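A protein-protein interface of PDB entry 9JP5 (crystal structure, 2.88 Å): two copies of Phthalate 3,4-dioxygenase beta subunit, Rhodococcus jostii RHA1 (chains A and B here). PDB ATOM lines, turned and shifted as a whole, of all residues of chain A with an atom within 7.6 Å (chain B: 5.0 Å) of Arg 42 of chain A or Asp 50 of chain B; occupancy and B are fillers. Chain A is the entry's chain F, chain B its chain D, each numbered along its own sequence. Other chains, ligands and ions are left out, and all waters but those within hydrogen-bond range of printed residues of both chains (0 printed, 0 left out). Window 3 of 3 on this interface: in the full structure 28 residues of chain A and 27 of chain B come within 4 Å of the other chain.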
ATOM      1  N   THR A  39     -14.672 -25.024  11.766  1.00  0.00           N
ATOM      2  CA  THR A  39     -14.149 -23.841  11.116  1.00  0.00           C
ATOM      3  C   THR A  39     -13.981 -22.790  12.212  1.00  0.00           C
ATOM      4  O   THR A  39     -14.228 -23.069  13.382  1.00  0.00           O
ATOM      5  CB  THR A  39     -15.028 -23.458   9.915  1.00  0.00           C
ATOM      6  OG1 THR A  39     -16.204 -22.827  10.425  1.00  0.00           O
ATOM      7  CG2 THR A  39     -15.376 -24.634   9.024  1.00  0.00           C
ATOM      8  N   PRO A  40     -13.470 -21.581  11.899  1.00  0.00           N
ATOM      9  CA  PRO A  40     -13.347 -20.517  12.898  1.00  0.00           C
ATOM     10  C   PRO A  40     -14.689 -20.028  13.450  1.00  0.00           C
ATOM     11  O   PRO A  40     -15.690 -20.005  12.729  1.00  0.00           O
ATOM     12  CB  PRO A  40     -12.671 -19.360  12.133  1.00  0.00           C
ATOM     13  CG  PRO A  40     -12.002 -20.028  10.946  1.00  0.00           C
ATOM     14  CD  PRO A  40     -12.903 -21.193  10.597  1.00  0.00           C
ATOM     15  N   LEU A  41     -14.686 -19.611  14.726  1.00  0.00           N
ATOM     16  CA  LEU A  41     -15.857 -19.005  15.337  1.00  0.00           C
ATOM     17  C   LEU A  41     -16.135 -17.669  14.665  1.00  0.00           C
ATOM     18  O   LEU A  41     -15.253 -17.071  14.047  1.00  0.00           O
ATOM     19  CB  LEU A  41     -15.641 -18.789  16.836  1.00  0.00           C
ATOM     20  CG  LEU A  41     -15.282 -20.025  17.665  1.00  0.00           C
ATOM     21  CD1 LEU A  41     -15.374 -19.729  19.159  1.00  0.00           C
ATOM     22  CD2 LEU A  41     -16.150 -21.215  17.313  1.00  0.00           C
ATOM     23  N   ARG A  42     -17.391 -17.232  14.786  1.00  0.00           N
ATOM     24  CA  ARG A  42     -17.777 -15.900  14.367  1.00  0.00           C
ATOM     25  C   ARG A  42     -17.091 -14.938  15.320  1.00  0.00           C
ATOM     26  O   ARG A  42     -16.645 -15.361  16.384  1.00  0.00           O
ATOM     27  CB  ARG A  42     -19.296 -15.710  14.400  1.00  0.00           C
ATOM     28  CG  ARG A  42     -20.073 -16.537  13.386  1.00  0.00           C
ATOM     29  CD  ARG A  42     -21.558 -16.227  13.487  1.00  0.00           C
ATOM     30  NE  ARG A  42     -22.361 -16.998  12.541  1.00  0.00           N
ATOM     31  CZ  ARG A  42     -22.445 -16.777  11.225  1.00  0.00           C
ATOM     32  NH1 ARG A  42     -22.002 -15.643  10.702  1.00  0.00           N
ATOM     33  NH2 ARG A  42     -23.021 -17.681  10.440  1.00  0.00           N
ATOM     34  N   PHE A  43     -17.015 -13.663  14.913  1.00  0.00           N
ATOM     35  CA  PHE A  43     -16.197 -12.683  15.616  1.00  0.00           C
ATOM     36  C   PHE A  43     -16.976 -12.037  16.764  1.00  0.00           C
ATOM     37  O   PHE A  43     -16.400 -11.275  17.531  1.00  0.00           O
ATOM     38  CB  PHE A  43     -15.607 -11.665  14.626  1.00  0.00           C
ATOM     39  CG  PHE A  43     -14.477 -12.175  13.754  1.00  0.00           C
ATOM     40  CD1 PHE A  43     -13.963 -13.459  13.917  1.00  0.00           C
ATOM     41  CD2 PHE A  43     -13.928 -11.367  12.762  1.00  0.00           C
ATOM     42  CE1 PHE A  43     -12.951 -13.929  13.097  1.00  0.00           C
ATOM     43  CE2 PHE A  43     -12.910 -11.840  11.952  1.00  0.00           C
ATOM     44  CZ  PHE A  43     -12.430 -13.120  12.119  1.00  0.00           C
ATOM     45  N   ASP A  44     -18.267 -12.376  16.901  1.00  0.00           N
ATOM     46  CA  ASP A  44     -19.068 -11.972  18.047  1.00  0.00           C
ATOM     47  C   ASP A  44     -19.194 -13.117  19.049  1.00  0.00           C
ATOM     48  O   ASP A  44     -19.784 -12.921  20.098  1.00  0.00           O
ATOM     49  CB  ASP A  44     -20.445 -11.465  17.608  1.00  0.00           C
ATOM     50  CG  ASP A  44     -21.376 -12.500  16.986  1.00  0.00           C
ATOM     51  OD1 ASP A  44     -20.912 -13.362  16.186  1.00  0.00           O
ATOM     52  OD2 ASP A  44     -22.583 -12.410  17.270  1.00  0.00           O
ATOM     53  N   ASP A  45     -18.648 -14.302  18.737  1.00  0.00           N
ATOM     54  CA  ASP A  45     -18.699 -15.445  19.635  1.00  0.00           C
ATOM     55  C   ASP A  45     -17.835 -15.171  20.862  1.00  0.00           C
ATOM     56  O   ASP A  45     -16.668 -14.836  20.733  1.00  0.00           O
ATOM     57  CB  ASP A  45     -18.232 -16.714  18.928  1.00  0.00           C
ATOM     58  CG  ASP A  45     -18.214 -17.962  19.789  1.00  0.00           C
ATOM     59  OD1 ASP A  45     -17.758 -17.882  20.934  1.00  0.00           O
ATOM     60  OD2 ASP A  45     -18.600 -19.018  19.276  1.00  0.00           O
ATOM     61  N   ARG A  46     -18.425 -15.363  22.048  1.00  0.00           N
ATOM     62  CA  ARG A  46     -17.823 -15.026  23.336  1.00  0.00           C
ATOM     63  C   ARG A  46     -16.387 -15.551  23.461  1.00  0.00           C
ATOM     64  O   ARG A  46     -15.511 -14.884  24.028  1.00  0.00           O
ATOM     65  CB  ARG A  46     -18.706 -15.596  24.455  1.00  0.00           C
ATOM     66  CG  ARG A  46     -18.139 -15.478  25.871  1.00  0.00           C
ATOM     67  CD  ARG A  46     -18.070 -14.068  26.449  1.00  0.00           C
ATOM     68  NE  ARG A  46     -19.136 -13.183  25.972  1.00  0.00           N
ATOM     69  CZ  ARG A  46     -18.999 -11.885  25.706  1.00  0.00           C
ATOM     70  NH1 ARG A  46     -17.890 -11.246  26.033  1.00  0.00           N
ATOM     71  NH2 ARG A  46     -19.993 -11.209  25.155  1.00  0.00           N
ATOM     72  N   ARG A  47     -16.158 -16.770  22.969  1.00  0.00           N
ATOM     73  CA  ARG A  47     -14.873 -17.435  23.138  1.00  0.00           C
ATOM     74  C   ARG A  47     -13.799 -16.757  22.272  1.00  0.00           C
ATOM     75  O   ARG A  47     -12.685 -16.507  22.737  1.00  0.00           O
ATOM     76  CB  ARG A  47     -15.059 -18.930  22.862  1.00  0.00           C
ATOM     77  CG  ARG A  47     -15.881 -19.638  23.930  1.00  0.00           C
ATOM     78  CD  ARG A  47     -16.532 -20.936  23.477  1.00  0.00           C
ATOM     79  NE  ARG A  47     -17.423 -20.723  22.338  1.00  0.00           N
ATOM     80  CZ  ARG A  47     -18.161 -21.662  21.745  1.00  0.00           C
ATOM     81  NH1 ARG A  47     -18.208 -22.897  22.222  1.00  0.00           N
ATOM     82  NH2 ARG A  47     -18.864 -21.353  20.671  1.00  0.00           N
ATOM     83  N   HIS A  48     -14.152 -16.418  21.022  1.00  0.00           N
ATOM     84  CA  HIS A  48     -13.310 -15.593  20.167  1.00  0.00           C
ATOM     85  C   HIS A  48     -12.964 -14.269  20.840  1.00  0.00           C
ATOM     86  O   HIS A  48     -11.798 -13.905  20.868  1.00  0.00           O
ATOM     87  CB  HIS A  48     -14.006 -15.291  18.838  1.00  0.00           C
ATOM     88  CG  HIS A  48     -13.276 -14.320  17.966  1.00  0.00           C
ATOM     89  ND1 HIS A  48     -12.277 -14.688  17.091  1.00  0.00           N
ATOM     90  CD2 HIS A  48     -13.463 -13.001  17.784  1.00  0.00           C
ATOM     91  CE1 HIS A  48     -11.865 -13.609  16.436  1.00  0.00           C
ATOM     92  NE2 HIS A  48     -12.570 -12.576  16.837  1.00  0.00           N
ATOM     93  N   LEU A  49     -13.985 -13.557  21.339  1.00  0.00           N
ATOM     94  CA  LEU A  49     -13.818 -12.249  21.963  1.00  0.00           C
ATOM     95  C   LEU A  49     -12.847 -12.356  23.134  1.00  0.00           C
ATOM     96  O   LEU A  49     -12.054 -11.450  23.363  1.00  0.00           O
ATOM     97  CB  LEU A  49     -15.173 -11.693  22.422  1.00  0.00           C
ATOM     98  CG  LEU A  49     -16.152 -11.344  21.295  1.00  0.00           C
ATOM     99  CD1 LEU A  49     -17.524 -10.969  21.835  1.00  0.00           C
ATOM    100  CD2 LEU A  49     -15.619 -10.218  20.415  1.00  0.00           C
ATOM    101  N   THR A 140     -10.291 -17.751  15.837  1.00  0.00           N
ATOM    102  CA  THR A 140     -10.380 -18.695  16.945  1.00  0.00           C
ATOM    103  C   THR A 140     -11.046 -20.000  16.510  1.00  0.00           C
ATOM    104  O   THR A 140     -11.916 -20.009  15.639  1.00  0.00           O
ATOM    105  CB  THR A 140     -11.156 -18.111  18.136  1.00  0.00           C
ATOM    106  OG1 THR A 140     -11.020 -16.687  18.163  1.00  0.00           O
ATOM    107  CG2 THR A 140     -10.716 -18.727  19.447  1.00  0.00           C
ATOM    108  N   ARG B  46     -23.921  -7.801  12.082  1.00  0.00           N
ATOM    109  CA  ARG B  46     -23.659  -9.130  11.540  1.00  0.00           C
ATOM    110  C   ARG B  46     -22.936  -9.046  10.191  1.00  0.00           C
ATOM    111  O   ARG B  46     -21.951  -9.761   9.958  1.00  0.00           O
ATOM    112  CB  ARG B  46     -24.992  -9.881  11.392  1.00  0.00           C
ATOM    113  CG  ARG B  46     -24.965 -11.232  10.668  1.00  0.00           C
ATOM    114  CD  ARG B  46     -24.368 -12.410  11.429  1.00  0.00           C
ATOM    115  NE  ARG B  46     -24.525 -12.338  12.880  1.00  0.00           N
ATOM    116  CZ  ARG B  46     -23.567 -12.591  13.780  1.00  0.00           C
ATOM    117  NH1 ARG B  46     -22.383 -13.077  13.424  1.00  0.00           N
ATOM    118  NH2 ARG B  46     -23.807 -12.377  15.062  1.00  0.00           N
ATOM    119  N   ARG B  47     -23.443  -8.174   9.308  1.00  0.00           N
ATOM    120  CA  ARG B  47     -22.922  -8.035   7.960  1.00  0.00           C
ATOM    121  C   ARG B  47     -21.479  -7.519   7.951  1.00  0.00           C
ATOM    122  O   ARG B  47     -20.727  -7.852   7.035  1.00  0.00           O
ATOM    123  CB  ARG B  47     -23.871  -7.144   7.164  1.00  0.00           C
ATOM    124  CG  ARG B  47     -25.228  -7.796   6.956  1.00  0.00           C
ATOM    125  CD  ARG B  47     -26.316  -6.804   6.603  1.00  0.00           C
ATOM    126  NE  ARG B  47     -26.476  -5.862   7.694  1.00  0.00           N
ATOM    127  CZ  ARG B  47     -27.277  -4.812   7.662  1.00  0.00           C
ATOM    128  NH1 ARG B  47     -28.083  -4.615   6.632  1.00  0.00           N
ATOM    129  NH2 ARG B  47     -27.261  -3.958   8.666  1.00  0.00           N
ATOM    130  N   HIS B  48     -21.092  -6.726   8.965  1.00  0.00           N
ATOM    131  CA  HIS B  48     -19.703  -6.319   9.144  1.00  0.00           C
ATOM    132  C   HIS B  48     -18.877  -7.505   9.639  1.00  0.00           C
ATOM    133  O   HIS B  48     -17.793  -7.765   9.130  1.00  0.00           O
ATOM    134  CB  HIS B  48     -19.577  -5.090  10.057  1.00  0.00           C
ATOM    135  CG  HIS B  48     -18.197  -4.815  10.583  1.00  0.00           C
ATOM    136  ND1 HIS B  48     -17.381  -3.851  10.033  1.00  0.00           N
ATOM    137  CD2 HIS B  48     -17.500  -5.354  11.601  1.00  0.00           C
ATOM    138  CE1 HIS B  48     -16.239  -3.822  10.701  1.00  0.00           C
ATOM    139  NE2 HIS B  48     -16.292  -4.723  11.658  1.00  0.00           N
ATOM    140  N   LEU B  49     -19.409  -8.235  10.617  1.00  0.00           N
ATOM    141  CA  LEU B  49     -18.699  -9.360  11.192  1.00  0.00           C
ATOM    142  C   LEU B  49     -18.423 -10.403  10.115  1.00  0.00           C
ATOM    143  O   LEU B  49     -17.396 -11.075  10.148  1.00  0.00           O
ATOM    144  CB  LEU B  49     -19.539  -9.954  12.321  1.00  0.00           C
ATOM    145  CG  LEU B  49     -19.802  -9.014  13.496  1.00  0.00           C
ATOM    146  CD1 LEU B  49     -20.719  -9.676  14.513  1.00  0.00           C
ATOM    147  CD2 LEU B  49     -18.503  -8.569  14.155  1.00  0.00           C
ATOM    148  N   ASP B  50     -19.329 -10.541   9.149  1.00  0.00           N
ATOM    149  CA  ASP B  50     -19.105 -11.514   8.096  1.00  0.00           C
ATOM    150  C   ASP B  50     -17.971 -11.026   7.196  1.00  0.00           C
ATOM    151  O   ASP B  50     -17.047 -11.785   6.891  1.00  0.00           O
ATOM    152  CB  ASP B  50     -20.399 -11.796   7.332  1.00  0.00           C
ATOM    153  CG  ASP B  50     -21.449 -12.565   8.121  1.00  0.00           C
ATOM    154  OD1 ASP B  50     -21.160 -12.967   9.287  1.00  0.00           O
ATOM    155  OD2 ASP B  50     -22.556 -12.748   7.562  1.00  0.00           O
ATOM    156  N   ALA B  51     -18.046  -9.753   6.800  1.00  0.00           N
ATOM    157  CA  ALA B  51     -17.066  -9.148   5.913  1.00  0.00           C
ATOM    158  C   ALA B  51     -15.659  -9.252   6.494  1.00  0.00           C
ATOM    159  O   ALA B  51     -14.723  -9.556   5.775  1.00  0.00           O
ATOM    160  CB  ALA B  51     -17.431  -7.707   5.683  1.00  0.00           C
ATOM    161  N   HIS B  52     -15.530  -8.976   7.792  1.00  0.00           N
ATOM    162  CA  HIS B  52     -14.267  -9.057   8.507  1.00  0.00           C
ATOM    163  C   HIS B  52     -13.781 -10.499   8.471  1.00  0.00           C
ATOM    164  O   HIS B  52     -12.685 -10.763   7.992  1.00  0.00           O
ATOM    165  CB  HIS B  52     -14.469  -8.527   9.932  1.00  0.00           C
ATOM    166  CG  HIS B  52     -13.254  -8.288  10.754  1.00  0.00           C
ATOM    167  ND1 HIS B  52     -11.996  -8.795  10.502  1.00  0.00           N
ATOM    168  CD2 HIS B  52     -13.156  -7.583  11.901  1.00  0.00           C
ATOM    169  CE1 HIS B  52     -11.163  -8.388  11.462  1.00  0.00           C
ATOM    170  NE2 HIS B  52     -11.843  -7.645  12.319  1.00  0.00           N
ATOM    171  N   GLN B  53     -14.642 -11.417   8.939  1.00  0.00           N
ATOM    172  CA  GLN B  53     -14.343 -12.845   8.971  1.00  0.00           C
ATOM    173  C   GLN B  53     -13.824 -13.308   7.608  1.00  0.00           C
ATOM    174  O   GLN B  53     -12.907 -14.123   7.544  1.00  0.00           O
ATOM    175  CB  GLN B  53     -15.581 -13.662   9.362  1.00  0.00           C
ATOM    176  CG  GLN B  53     -15.791 -13.842  10.865  1.00  0.00           C
ATOM    177  CD  GLN B  53     -17.243 -14.054  11.252  1.00  0.00           C
ATOM    178  OE1 GLN B  53     -17.746 -13.496  12.229  1.00  0.00           O
ATOM    179  NE2 GLN B  53     -17.943 -14.873  10.483  1.00  0.00           N
ATOM    180  N   PHE B  54     -14.429 -12.810   6.526  1.00  0.00           N
ATOM    181  CA  PHE B  54     -14.020 -13.199   5.191  1.00  0.00           C
ATOM    182  C   PHE B  54     -12.564 -12.810   4.932  1.00  0.00           C
ATOM    183  O   PHE B  54     -11.806 -13.603   4.365  1.00  0.00           O
ATOM    184  CB  PHE B  54     -14.933 -12.544   4.159  1.00  0.00           C
ATOM    185  CG  PHE B  54     -14.575 -12.868   2.735  1.00  0.00           C
ATOM    186  CD1 PHE B  54     -15.011 -14.038   2.139  1.00  0.00           C
ATOM    187  CD2 PHE B  54     -13.821 -11.993   1.976  1.00  0.00           C
ATOM    188  CE1 PHE B  54     -14.703 -14.328   0.815  1.00  0.00           C
ATOM    189  CE2 PHE B  54     -13.500 -12.289   0.657  1.00  0.00           C
ATOM    190  CZ  PHE B  54     -13.953 -13.450   0.073  1.00  0.00           C
ATOM    191  N   TRP B 185     -20.360 -15.590   1.439  1.00  0.00           N
ATOM    192  CA  TRP B 185     -19.888 -14.359   0.819  1.00  0.00           C
ATOM    193  C   TRP B 185     -18.754 -14.642  -0.159  1.00  0.00           C
ATOM    194  O   TRP B 185     -17.944 -15.544   0.063  1.00  0.00           O
ATOM    195  CB  TRP B 185     -19.399 -13.391   1.898  1.00  0.00           C
ATOM    196  CG  TRP B 185     -20.519 -12.813   2.717  1.00  0.00           C
ATOM    197  CD1 TRP B 185     -20.844 -13.102   4.008  1.00  0.00           C
ATOM    198  CD2 TRP B 185     -21.450 -11.807   2.275  1.00  0.00           C
ATOM    199  NE1 TRP B 185     -21.914 -12.347   4.399  1.00  0.00           N
ATOM    200  CE2 TRP B 185     -22.306 -11.548   3.359  1.00  0.00           C
ATOM    201  CE3 TRP B 185     -21.628 -11.114   1.082  1.00  0.00           C
ATOM    202  CZ2 TRP B 185     -23.335 -10.623   3.281  1.00  0.00           C
ATOM    203  CZ3 TRP B 185     -22.644 -10.194   1.009  1.00  0.00           C
ATOM    204  CH2 TRP B 185     -23.480  -9.950   2.094  1.00  0.00           C
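OD1 of Asp 50 of chain B lies within salt-bridge range of NH1 of Arg 42 of chain A (3.1 Å).
The side-chain amide oxygen (OE1) of Gln 53 of chain B sits at hydrogen-bond distance from the backbone NH (N) of Phe 43 of chain A (2.8 Å).
NH2 of Arg 46 of chain B lies within salt-bridge range of OD2 of Asp 44 of chain A (2.5 Å).
OE1 of Gln 53 of chain B lies close to O of Leu 49 of chain B (3.2 Å).
OD2 of Asp 50 of chain B lies within hydrogen-bond range of NE1 of Trp 185 of chain B (3.3 Å).
Among the printed residues, merely in contact across the chains: Arg 42 of chain A with Gln 53 of chain B, Arg 42 of chain A with Arg 46 of chain B, Phe 43 of chain A with His 52 of chain B and Asp 44 of chain A with Leu 49 of chain B.
Of chain B, only Arg 46, Asp 50 and Gln 53 come within 4 Å of Arg 42 of chain A.
Of chain A, only Arg 42 (3.1 Å) comes within 4 Å of Asp 50 of chain B.
Of the printed residues of chain A, Gln 53 of chain B touches Arg 42 (3.2 Å) and Phe 43 (2.8 Å).
Of the printed residues of chain B, Asp 44 of chain A touches Arg 46 (2.5 Å) and Leu 49 (3.6 Å).
Of the printed residues of chain B, Phe 43 of chain A touches His 52 (3.5 Å) and Gln 53 (2.8 Å).
Arg 47 of chain A touches none of the printed residues of chain B.
The nearest residue of chain A that does not touch Asp 50 of chain B is Phe 43 of chain A (6.5 Å).
The nearest printed residue of chain A that does not touch Gln 53 of chain B is Leu 41 of chain A (4.6 Å).
Of the 12 printed residues of chain A, 3 touch a printed residue of chain B.
Hydrophobic or aromatic side chains of chain A that line the printed part of chain B: Phe 43.
Of the 10 printed residues of chain B, 5 touch a printed residue of chain A.
Among the printed residues, Asp or Glu carboxylates within 4 Å of a Lys or Arg side-chain nitrogen of the other chain: Arg 42 of chain A with Asp 50 of chain B (3.1 Å) and Asp 44 of chain A with Arg 46 of chain B (2.5 Å).
Positions printed for both chains: 46, 47, 48 and 49.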
